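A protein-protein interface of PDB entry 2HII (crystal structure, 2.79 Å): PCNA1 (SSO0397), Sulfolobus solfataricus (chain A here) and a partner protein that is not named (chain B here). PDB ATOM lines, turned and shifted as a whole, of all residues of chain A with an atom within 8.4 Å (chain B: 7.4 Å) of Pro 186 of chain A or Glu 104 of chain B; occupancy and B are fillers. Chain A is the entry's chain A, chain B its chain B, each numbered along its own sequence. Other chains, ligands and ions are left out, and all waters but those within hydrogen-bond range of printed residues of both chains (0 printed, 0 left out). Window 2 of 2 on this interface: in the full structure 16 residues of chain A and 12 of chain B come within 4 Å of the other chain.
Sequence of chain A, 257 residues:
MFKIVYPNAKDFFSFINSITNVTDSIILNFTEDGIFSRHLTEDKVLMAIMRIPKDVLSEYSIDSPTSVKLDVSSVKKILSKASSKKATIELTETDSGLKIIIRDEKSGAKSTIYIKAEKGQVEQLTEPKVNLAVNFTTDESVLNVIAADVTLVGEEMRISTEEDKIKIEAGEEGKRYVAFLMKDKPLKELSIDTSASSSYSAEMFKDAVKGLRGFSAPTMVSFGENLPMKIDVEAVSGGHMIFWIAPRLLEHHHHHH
The backbone carbonyl oxygen (O) of Thr 106 of chain B is in hydrogen-bond range of the backbone NH (N) of Phe 180 of chain A (3.4 Å).
The backbone carbonyl oxygen (O) of Glu 104 of chain B lies close to the backbone nitrogen (N) of Pro 186 of chain A, at 3.4 Å.
Of the 21 printed residues of chain A, 5 touch a printed residue of chain B.
Hydrophobic or aromatic side chains of chain A that line the printed part of chain B: Val 145, Leu 181 and Pro 186.
Of the 10 printed residues of chain B, 4 touch a printed residue of chain A.
Hydrophobic or aromatic side chains of chain B within 4 Å of the printed part of chain A: Phe 105.
Among the printed residues, 8 pairs touch across the chains.
CG1 of Val 145 of chain A touches NH1 of Arg 107 of chain B (3.7 Å).
Phe 105 of chain B touches Phe 180 of chain A.
Phe 105 of chain B touches Leu 181 of chain A.
Lys 185 of chain A touches Glu 104 of chain B.
Phe 105 of chain B touches Lys 185 of chain A (CB to O, 3.8 Å).
CD of Pro 186 of chain A touches CB of Phe 105 of chain B, 3.6 Å away.
OD2 of Asp 86 of chain B is in salt-bridge range of NH2 of Arg 107 of chain B.
N of Phe 101 of chain B lies within hydrogen-bond range of O of Arg 107 of chain B, at 2.6 Å.
N of Leu 181 of chain A is in hydrogen-bond range of O of Ile 166 of chain A (2.8 Å).
Pro 186 of chain A touches just these residues of chain B: Glu 104 and Phe 105.
Of chain A, only Lys 185 (3.3 Å) and Pro 186 (3.4 Å) come within 4 Å of Glu 104 of chain B.
No residue of chain A comes within 4 Å of Gly 103 of chain B.
Of the printed residues of chain B, Phe 180 of chain A touches Phe 105 and Thr 106.
Printed residues of chain B within 4 Å of Lys 185 of chain A: Glu 104 (3.3 Å) and Phe 105 (3.8 Å).
Of the printed residues of chain B, Val 145 of chain A touches Arg 107.
Printed residues of chain A within 4 Å of Arg 107 of chain B: Val 145 (3.7 Å).
Phe 136 of chain A touches none of the printed residues of chain B.
The nearest residue of chain B that does not touch Pro 186 of chain A is Thr 106 of chain B (6.5 Å).
The nearest printed residue of chain B that does not touch Lys 185 of chain A is Gly 103 of chain B (5.2 Å).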
ATOM      1  N   PHE A 136     -11.181 -12.634  36.617  1.00  0.00           N
ATOM      2  CA  PHE A 136     -11.507 -11.679  35.548  1.00  0.00           C
ATOM      3  C   PHE A 136     -12.967 -11.288  35.566  1.00  0.00           C
ATOM      4  O   PHE A 136     -13.830 -12.083  35.958  1.00  0.00           O
ATOM      5  CB  PHE A 136     -11.052 -12.149  34.151  1.00  0.00           C
ATOM      6  CG  PHE A 136     -11.725 -13.413  33.642  1.00  0.00           C
ATOM      7  CD1 PHE A 136     -12.777 -13.339  32.741  1.00  0.00           C
ATOM      8  CD2 PHE A 136     -11.256 -14.675  34.010  1.00  0.00           C
ATOM      9  CE1 PHE A 136     -13.371 -14.490  32.239  1.00  0.00           C
ATOM     10  CE2 PHE A 136     -11.844 -15.831  33.519  1.00  0.00           C
ATOM     11  CZ  PHE A 136     -12.907 -15.741  32.631  1.00  0.00           C
ATOM     12  N   THR A 137     -13.250 -10.048  35.185  1.00  0.00           N
ATOM     13  CA  THR A 137     -14.636  -9.602  35.132  1.00  0.00           C
ATOM     14  C   THR A 137     -15.019  -9.114  33.740  1.00  0.00           C
ATOM     15  O   THR A 137     -14.286  -8.350  33.120  1.00  0.00           O
ATOM     16  CB  THR A 137     -15.035  -8.616  36.300  1.00  0.00           C
ATOM     17  OG1 THR A 137     -15.699  -7.456  35.779  1.00  0.00           O
ATOM     18  CG2 THR A 137     -13.836  -8.186  37.135  1.00  0.00           C
ATOM     19  N   THR A 138     -16.153  -9.604  33.252  1.00  0.00           N
ATOM     20  CA  THR A 138     -16.601  -9.308  31.908  1.00  0.00           C
ATOM     21  C   THR A 138     -18.139  -9.293  31.785  1.00  0.00           C
ATOM     22  O   THR A 138     -18.808  -8.742  32.654  1.00  0.00           O
ATOM     23  CB  THR A 138     -15.863 -10.194  30.847  1.00  0.00           C
ATOM     24  OG1 THR A 138     -16.281  -9.824  29.525  1.00  0.00           O
ATOM     25  CG2 THR A 138     -16.074 -11.692  31.085  1.00  0.00           C
ATOM     26  N   ASP A 139     -18.685  -9.901  30.730  1.00  0.00           N
ATOM     27  CA  ASP A 139     -20.045  -9.651  30.265  1.00  0.00           C
ATOM     28  C   ASP A 139     -20.707 -10.987  30.029  1.00  0.00           C
ATOM     29  O   ASP A 139     -20.067 -11.910  29.518  1.00  0.00           O
ATOM     30  CB  ASP A 139     -19.938  -8.921  28.936  1.00  0.00           C
ATOM     31  CG  ASP A 139     -21.181  -8.173  28.573  1.00  0.00           C
ATOM     32  OD1 ASP A 139     -22.273  -8.803  28.515  1.00  0.00           O
ATOM     33  OD2 ASP A 139     -21.046  -6.948  28.305  1.00  0.00           O
ATOM     34  N   SER A 141     -22.607 -11.587  27.746  1.00  0.00           N
ATOM     35  CA  SER A 141     -22.536 -11.750  26.299  1.00  0.00           C
ATOM     36  C   SER A 141     -21.235 -12.429  25.881  1.00  0.00           C
ATOM     37  O   SER A 141     -21.249 -13.346  25.057  1.00  0.00           O
ATOM     38  CB  SER A 141     -22.668 -10.405  25.592  1.00  0.00           C
ATOM     39  OG  SER A 141     -21.466  -9.686  25.707  1.00  0.00           O
ATOM     40  N   VAL A 142     -20.121 -11.980  26.457  1.00  0.00           N
ATOM     41  CA  VAL A 142     -18.817 -12.575  26.181  1.00  0.00           C
ATOM     42  C   VAL A 142     -18.822 -14.050  26.557  1.00  0.00           C
ATOM     43  O   VAL A 142     -18.385 -14.901  25.783  1.00  0.00           O
ATOM     44  CB  VAL A 142     -17.665 -11.835  26.918  1.00  0.00           C
ATOM     45  CG1 VAL A 142     -16.357 -12.600  26.795  1.00  0.00           C
ATOM     46  CG2 VAL A 142     -17.492 -10.434  26.365  1.00  0.00           C
ATOM     47  N   LEU A 143     -19.331 -14.346  27.743  1.00  0.00           N
ATOM     48  CA  LEU A 143     -19.369 -15.716  28.215  1.00  0.00           C
ATOM     49  C   LEU A 143     -20.202 -16.602  27.287  1.00  0.00           C
ATOM     50  O   LEU A 143     -19.803 -17.720  26.972  1.00  0.00           O
ATOM     51  CB  LEU A 143     -19.888 -15.779  29.643  1.00  0.00           C
ATOM     52  CG  LEU A 143     -19.005 -15.490  30.873  1.00  0.00           C
ATOM     53  CD1 LEU A 143     -17.505 -15.667  30.614  1.00  0.00           C
ATOM     54  CD2 LEU A 143     -19.295 -14.128  31.467  1.00  0.00           C
ATOM     55  N   VAL A 145     -20.704 -16.251  24.062  1.00  0.00           N
ATOM     56  CA  VAL A 145     -19.959 -16.506  22.841  1.00  0.00           C
ATOM     57  C   VAL A 145     -19.029 -17.676  23.094  1.00  0.00           C
ATOM     58  O   VAL A 145     -18.933 -18.596  22.291  1.00  0.00           O
ATOM     59  CB  VAL A 145     -19.121 -15.282  22.396  1.00  0.00           C
ATOM     60  CG1 VAL A 145     -18.526 -15.506  21.018  1.00  0.00           C
ATOM     61  CG2 VAL A 145     -19.955 -14.018  22.401  1.00  0.00           C
ATOM     62  N   ILE A 146     -18.363 -17.643  24.239  1.00  0.00           N
ATOM     63  CA  ILE A 146     -17.362 -18.639  24.558  1.00  0.00           C
ATOM     64  C   ILE A 146     -18.028 -19.999  24.676  1.00  0.00           C
ATOM     65  O   ILE A 146     -17.603 -20.960  24.038  1.00  0.00           O
ATOM     66  CB  ILE A 146     -16.568 -18.263  25.825  1.00  0.00           C
ATOM     67  CG1 ILE A 146     -15.757 -16.977  25.574  1.00  0.00           C
ATOM     68  CG2 ILE A 146     -15.636 -19.406  26.223  1.00  0.00           C
ATOM     69  CD1 ILE A 146     -15.057 -16.414  26.795  1.00  0.00           C
ATOM     70  N   ILE A 166      -5.895 -14.599  29.514  1.00  0.00           N
ATOM     71  CA  ILE A 166      -6.584 -15.856  29.770  1.00  0.00           C
ATOM     72  C   ILE A 166      -6.728 -16.625  28.458  1.00  0.00           C
ATOM     73  O   ILE A 166      -7.087 -16.054  27.427  1.00  0.00           O
ATOM     74  CB  ILE A 166      -7.918 -15.661  30.525  1.00  0.00           C
ATOM     75  CG1 ILE A 166      -7.681 -15.719  32.038  1.00  0.00           C
ATOM     76  CG2 ILE A 166      -8.931 -16.735  30.169  1.00  0.00           C
ATOM     77  CD1 ILE A 166      -7.351 -14.399  32.672  1.00  0.00           C
ATOM     78  N   PHE A 180      -8.137 -16.194  23.275  1.00  0.00           N
ATOM     79  CA  PHE A 180      -7.305 -15.403  24.174  1.00  0.00           C
ATOM     80  C   PHE A 180      -8.082 -14.164  24.602  1.00  0.00           C
ATOM     81  O   PHE A 180      -8.551 -13.397  23.754  1.00  0.00           O
ATOM     82  CB  PHE A 180      -6.001 -14.993  23.477  1.00  0.00           C
ATOM     83  CG  PHE A 180      -4.995 -16.112  23.331  1.00  0.00           C
ATOM     84  CD1 PHE A 180      -4.981 -16.913  22.197  1.00  0.00           C
ATOM     85  CD2 PHE A 180      -4.049 -16.355  24.329  1.00  0.00           C
ATOM     86  CE1 PHE A 180      -4.040 -17.942  22.059  1.00  0.00           C
ATOM     87  CE2 PHE A 180      -3.109 -17.382  24.204  1.00  0.00           C
ATOM     88  CZ  PHE A 180      -3.106 -18.176  23.062  1.00  0.00           C
ATOM     89  N   LEU A 181      -8.233 -13.986  25.910  1.00  0.00           N
ATOM     90  CA  LEU A 181      -8.898 -12.807  26.465  1.00  0.00           C
ATOM     91  C   LEU A 181      -7.886 -11.990  27.216  1.00  0.00           C
ATOM     92  O   LEU A 181      -7.024 -12.556  27.887  1.00  0.00           O
ATOM     93  CB  LEU A 181      -9.975 -13.196  27.475  1.00  0.00           C
ATOM     94  CG  LEU A 181     -11.106 -14.167  27.188  1.00  0.00           C
ATOM     95  CD1 LEU A 181     -11.746 -14.452  28.512  1.00  0.00           C
ATOM     96  CD2 LEU A 181     -12.102 -13.570  26.241  1.00  0.00           C
ATOM     97  N   MET A 182      -8.012 -10.666  27.135  1.00  0.00           N
ATOM     98  CA  MET A 182      -7.175  -9.756  27.930  1.00  0.00           C
ATOM     99  C   MET A 182      -7.824  -8.412  28.258  1.00  0.00           C
ATOM    100  O   MET A 182      -8.941  -8.122  27.827  1.00  0.00           O
ATOM    101  CB  MET A 182      -5.830  -9.532  27.262  1.00  0.00           C
ATOM    102  CG  MET A 182      -5.910  -8.772  25.990  1.00  0.00           C
ATOM    103  SD  MET A 182      -4.415  -9.376  24.948  1.00  0.00           S
ATOM    104  CE  MET A 182      -3.755  -7.623  24.304  1.00  0.00           C
ATOM    105  N   LYS A 183      -7.101  -7.596  29.020  1.00  0.00           N
ATOM    106  CA  LYS A 183      -7.625  -6.332  29.527  1.00  0.00           C
ATOM    107  C   LYS A 183      -8.036  -5.407  28.400  1.00  0.00           C
ATOM    108  O   LYS A 183      -7.225  -5.054  27.549  1.00  0.00           O
ATOM    109  CB  LYS A 183      -6.606  -5.634  30.438  1.00  0.00           C
ATOM    110  CG  LYS A 183      -7.133  -4.353  31.078  1.00  0.00           C
ATOM    111  CD  LYS A 183      -6.445  -4.064  32.382  1.00  0.00           C
ATOM    112  CE  LYS A 183      -7.464  -3.697  33.435  1.00  0.00           C
ATOM    113  NZ  LYS A 183      -7.022  -4.191  34.764  1.00  0.00           N
ATOM    114  N   ASP A 184      -9.312  -5.031  28.424  1.00  0.00           N
ATOM    115  CA  ASP A 184      -9.919  -4.142  27.437  1.00  0.00           C
ATOM    116  C   ASP A 184     -10.072  -4.809  26.075  1.00  0.00           C
ATOM    117  O   ASP A 184     -10.542  -4.182  25.122  1.00  0.00           O
ATOM    118  CB  ASP A 184      -9.142  -2.831  27.334  1.00  0.00           C
ATOM    119  CG  ASP A 184      -8.651  -2.352  28.681  1.00  0.00           C
ATOM    120  OD1 ASP A 184      -9.446  -2.384  29.643  1.00  0.00           O
ATOM    121  OD2 ASP A 184      -7.465  -1.974  28.783  1.00  0.00           O
ATOM    122  N   LYS A 185      -9.680  -6.080  25.997  1.00  0.00           N
ATOM    123  CA  LYS A 185      -9.894  -6.893  24.811  1.00  0.00           C
ATOM    124  C   LYS A 185     -10.200  -8.339  25.204  1.00  0.00           C
ATOM    125  O   LYS A 185      -9.373  -9.228  24.969  1.00  0.00           O
ATOM    126  CB  LYS A 185      -8.678  -6.822  23.873  1.00  0.00           C
ATOM    127  CG  LYS A 185      -8.720  -5.684  22.843  1.00  0.00           C
ATOM    128  CD  LYS A 185      -7.396  -5.571  22.074  1.00  0.00           C
ATOM    129  CE  LYS A 185      -7.412  -4.447  21.021  1.00  0.00           C
ATOM    130  NZ  LYS A 185      -7.342  -3.072  21.604  1.00  0.00           N
ATOM    131  N   PRO A 186     -11.393  -8.587  25.790  1.00  0.00           N
ATOM    132  CA  PRO A 186     -12.487  -7.685  26.162  1.00  0.00           C
ATOM    133  C   PRO A 186     -12.679  -7.471  27.673  1.00  0.00           C
ATOM    134  O   PRO A 186     -13.658  -6.852  28.070  1.00  0.00           O
ATOM    135  CB  PRO A 186     -13.696  -8.464  25.668  1.00  0.00           C
ATOM    136  CG  PRO A 186     -13.308  -9.934  26.013  1.00  0.00           C
ATOM    137  CD  PRO A 186     -11.779  -9.984  26.053  1.00  0.00           C
ATOM    138  N   LEU A 187     -11.779  -7.999  28.498  1.00  0.00           N
ATOM    139  CA  LEU A 187     -11.974  -8.040  29.954  1.00  0.00           C
ATOM    140  C   LEU A 187     -12.106  -6.660  30.581  1.00  0.00           C
ATOM    141  O   LEU A 187     -11.411  -5.723  30.186  1.00  0.00           O
ATOM    142  CB  LEU A 187     -10.830  -8.797  30.632  1.00  0.00           C
ATOM    143  CG  LEU A 187     -10.623 -10.251  30.206  1.00  0.00           C
ATOM    144  CD1 LEU A 187      -9.385 -10.857  30.830  1.00  0.00           C
ATOM    145  CD2 LEU A 187     -11.850 -11.069  30.532  1.00  0.00           C
ATOM    146  N   LYS A 188     -12.999  -6.542  31.558  1.00  0.00           N
ATOM    147  CA  LYS A 188     -13.212  -5.272  32.243  1.00  0.00           C
ATOM    148  C   LYS A 188     -12.177  -5.103  33.344  1.00  0.00           C
ATOM    149  O   LYS A 188     -11.643  -4.010  33.549  1.00  0.00           O
ATOM    150  CB  LYS A 188     -14.630  -5.179  32.805  1.00  0.00           C
ATOM    151  CG  LYS A 188     -15.714  -5.549  31.794  1.00  0.00           C
ATOM    152  CD  LYS A 188     -17.100  -5.112  32.228  1.00  0.00           C
ATOM    153  CE  LYS A 188     -17.973  -4.936  31.008  1.00  0.00           C
ATOM    154  NZ  LYS A 188     -19.260  -4.275  31.339  1.00  0.00           N
ATOM    155  N   GLU A 189     -11.894  -6.198  34.046  1.00  0.00           N
ATOM    156  CA  GLU A 189     -10.830  -6.226  35.038  1.00  0.00           C
ATOM    157  C   GLU A 189     -10.132  -7.569  34.917  1.00  0.00           C
ATOM    158  O   GLU A 189     -10.754  -8.552  34.511  1.00  0.00           O
ATOM    159  CB  GLU A 189     -11.409  -6.050  36.445  1.00  0.00           C
ATOM    160  CG  GLU A 189     -10.580  -5.161  37.365  1.00  0.00           C
ATOM    161  CD  GLU A 189     -10.718  -3.667  37.032  1.00  0.00           C
ATOM    162  OE1 GLU A 189     -11.873  -3.171  36.992  1.00  0.00           O
ATOM    163  OE2 GLU A 189      -9.677  -2.987  36.820  1.00  0.00           O
ATOM    164  N   LEU A 190      -8.842  -7.605  35.256  1.00  0.00           N
ATOM    165  CA  LEU A 190      -8.071  -8.847  35.249  1.00  0.00           C
ATOM    166  C   LEU A 190      -7.016  -8.875  36.352  1.00  0.00           C
ATOM    167  O   LEU A 190      -6.179  -7.975  36.445  1.00  0.00           O
ATOM    168  CB  LEU A 190      -7.384  -9.039  33.899  1.00  0.00           C
ATOM    169  CG  LEU A 190      -6.908 -10.425  33.450  1.00  0.00           C
ATOM    170  CD1 LEU A 190      -5.570 -10.292  32.749  1.00  0.00           C
ATOM    171  CD2 LEU A 190      -6.821 -11.461  34.574  1.00  0.00           C
ATOM    172  N   LEU B  83     -19.208 -12.523  14.963  1.00  0.00           N
ATOM    173  CA  LEU B  83     -19.820 -11.398  15.664  1.00  0.00           C
ATOM    174  C   LEU B  83     -19.848 -10.184  14.742  1.00  0.00           C
ATOM    175  O   LEU B  83     -18.990 -10.047  13.857  1.00  0.00           O
ATOM    176  CB  LEU B  83     -19.078 -11.068  16.972  1.00  0.00           C
ATOM    177  CG  LEU B  83     -19.054 -12.065  18.142  1.00  0.00           C
ATOM    178  CD1 LEU B  83     -18.840 -11.312  19.454  1.00  0.00           C
ATOM    179  CD2 LEU B  83     -20.318 -12.901  18.232  1.00  0.00           C
ATOM    180  N   ASP B  85     -19.076  -6.952  14.269  1.00  0.00           N
ATOM    181  CA  ASP B  85     -17.990  -6.112  13.780  1.00  0.00           C
ATOM    182  C   ASP B  85     -16.629  -6.796  13.703  1.00  0.00           C
ATOM    183  O   ASP B  85     -15.604  -6.121  13.785  1.00  0.00           O
ATOM    184  CB  ASP B  85     -17.871  -4.855  14.651  1.00  0.00           C
ATOM    185  CG  ASP B  85     -18.965  -3.845  14.373  1.00  0.00           C
ATOM    186  OD1 ASP B  85     -19.504  -3.285  15.348  1.00  0.00           O
ATOM    187  OD2 ASP B  85     -19.286  -3.611  13.185  1.00  0.00           O
ATOM    188  N   ASP B  86     -16.575  -8.113  13.547  1.00  0.00           N
ATOM    189  CA  ASP B  86     -15.248  -8.728  13.595  1.00  0.00           C
ATOM    190  C   ASP B  86     -14.742  -9.277  12.269  1.00  0.00           C
ATOM    191  O   ASP B  86     -15.528  -9.610  11.391  1.00  0.00           O
ATOM    192  CB  ASP B  86     -15.078  -9.695  14.789  1.00  0.00           C
ATOM    193  CG  ASP B  86     -15.955 -10.909  14.702  1.00  0.00           C
ATOM    194  OD1 ASP B  86     -16.480 -11.197  13.606  1.00  0.00           O
ATOM    195  OD2 ASP B  86     -16.100 -11.582  15.742  1.00  0.00           O
ATOM    196  N   PHE B 101     -11.233 -15.220  14.052  1.00  0.00           N
ATOM    197  CA  PHE B 101     -12.050 -14.024  14.185  1.00  0.00           C
ATOM    198  C   PHE B 101     -11.367 -12.998  15.067  1.00  0.00           C
ATOM    199  O   PHE B 101     -10.743 -13.346  16.062  1.00  0.00           O
ATOM    200  CB  PHE B 101     -13.404 -14.373  14.775  1.00  0.00           C
ATOM    201  CG  PHE B 101     -14.182 -15.345  13.958  1.00  0.00           C
ATOM    202  CD1 PHE B 101     -14.394 -16.636  14.414  1.00  0.00           C
ATOM    203  CD2 PHE B 101     -14.706 -14.974  12.727  1.00  0.00           C
ATOM    204  CE1 PHE B 101     -15.128 -17.550  13.668  1.00  0.00           C
ATOM    205  CE2 PHE B 101     -15.440 -15.883  11.963  1.00  0.00           C
ATOM    206  CZ  PHE B 101     -15.652 -17.175  12.438  1.00  0.00           C
ATOM    207  N   ASP B 102     -11.501 -11.730  14.707  1.00  0.00           N
ATOM    208  CA  ASP B 102     -10.808 -10.687  15.422  1.00  0.00           C
ATOM    209  C   ASP B 102     -11.693  -9.473  15.608  1.00  0.00           C
ATOM    210  O   ASP B 102     -11.954  -8.731  14.660  1.00  0.00           O
ATOM    211  CB  ASP B 102      -9.533 -10.319  14.679  1.00  0.00           C
ATOM    212  CG  ASP B 102      -8.456  -9.867  15.603  1.00  0.00           C
ATOM    213  OD1 ASP B 102      -7.427 -10.568  15.670  1.00  0.00           O
ATOM    214  OD2 ASP B 102      -8.644  -8.833  16.285  1.00  0.00           O
ATOM    215  N   GLY B 103     -12.154  -9.287  16.841  1.00  0.00           N
ATOM    216  CA  GLY B 103     -13.035  -8.189  17.204  1.00  0.00           C
ATOM    217  C   GLY B 103     -12.864  -7.850  18.664  1.00  0.00           C
ATOM    218  O   GLY B 103     -11.802  -7.377  19.074  1.00  0.00           O
ATOM    219  N   GLU B 104     -13.906  -8.102  19.455  1.00  0.00           N
ATOM    220  CA  GLU B 104     -13.858  -7.851  20.900  1.00  0.00           C
ATOM    221  C   GLU B 104     -12.746  -8.657  21.555  1.00  0.00           C
ATOM    222  O   GLU B 104     -12.160  -8.213  22.531  1.00  0.00           O
ATOM    223  CB  GLU B 104     -15.201  -8.154  21.574  1.00  0.00           C
ATOM    224  CG  GLU B 104     -16.331  -7.208  21.176  1.00  0.00           C
ATOM    225  CD  GLU B 104     -17.523  -7.253  22.122  1.00  0.00           C
ATOM    226  OE1 GLU B 104     -17.355  -7.670  23.293  1.00  0.00           O
ATOM    227  OE2 GLU B 104     -18.631  -6.850  21.693  1.00  0.00           O
ATOM    228  N   PHE B 105     -12.480  -9.843  21.006  1.00  0.00           N
ATOM    229  CA  PHE B 105     -11.317 -10.664  21.363  1.00  0.00           C
ATOM    230  C   PHE B 105     -11.008 -11.659  20.234  1.00  0.00           C
ATOM    231  O   PHE B 105     -11.864 -11.942  19.400  1.00  0.00           O
ATOM    232  CB  PHE B 105     -11.518 -11.374  22.716  1.00  0.00           C
ATOM    233  CG  PHE B 105     -12.620 -12.399  22.721  1.00  0.00           C
ATOM    234  CD1 PHE B 105     -12.324 -13.745  22.885  1.00  0.00           C
ATOM    235  CD2 PHE B 105     -13.945 -12.022  22.552  1.00  0.00           C
ATOM    236  CE1 PHE B 105     -13.326 -14.692  22.884  1.00  0.00           C
ATOM    237  CE2 PHE B 105     -14.945 -12.965  22.540  1.00  0.00           C
ATOM    238  CZ  PHE B 105     -14.637 -14.301  22.708  1.00  0.00           C
ATOM    239  N   THR B 106      -9.784 -12.174  20.213  1.00  0.00           N
ATOM    240  CA  THR B 106      -9.342 -13.078  19.162  1.00  0.00           C
ATOM    241  C   THR B 106      -9.825 -14.502  19.409  1.00  0.00           C
ATOM    242  O   THR B 106      -9.751 -15.008  20.524  1.00  0.00           O
ATOM    243  CB  THR B 106      -7.817 -13.063  19.027  1.00  0.00           C
ATOM    244  OG1 THR B 106      -7.330 -11.756  19.351  1.00  0.00           O
ATOM    245  CG2 THR B 106      -7.399 -13.416  17.603  1.00  0.00           C
ATOM    246  N   ARG B 107     -10.318 -15.135  18.351  1.00  0.00           N
ATOM    247  CA  ARG B 107     -10.910 -16.462  18.418  1.00  0.00           C
ATOM    248  C   ARG B 107     -10.522 -17.235  17.184  1.00  0.00           C
ATOM    249  O   ARG B 107     -10.704 -16.740  16.076  1.00  0.00           O
ATOM    250  CB  ARG B 107     -12.430 -16.347  18.412  1.00  0.00           C
ATOM    251  CG  ARG B 107     -13.027 -15.798  19.673  1.00  0.00           C
ATOM    252  CD  ARG B 107     -14.529 -15.785  19.574  1.00  0.00           C
ATOM    253  NE  ARG B 107     -14.976 -14.928  18.485  1.00  0.00           N
ATOM    254  CZ  ARG B 107     -16.028 -15.190  17.728  1.00  0.00           C
ATOM    255  NH1 ARG B 107     -16.733 -16.292  17.927  1.00  0.00           N
ATOM    256  NH2 ARG B 107     -16.370 -14.355  16.760  1.00  0.00           N
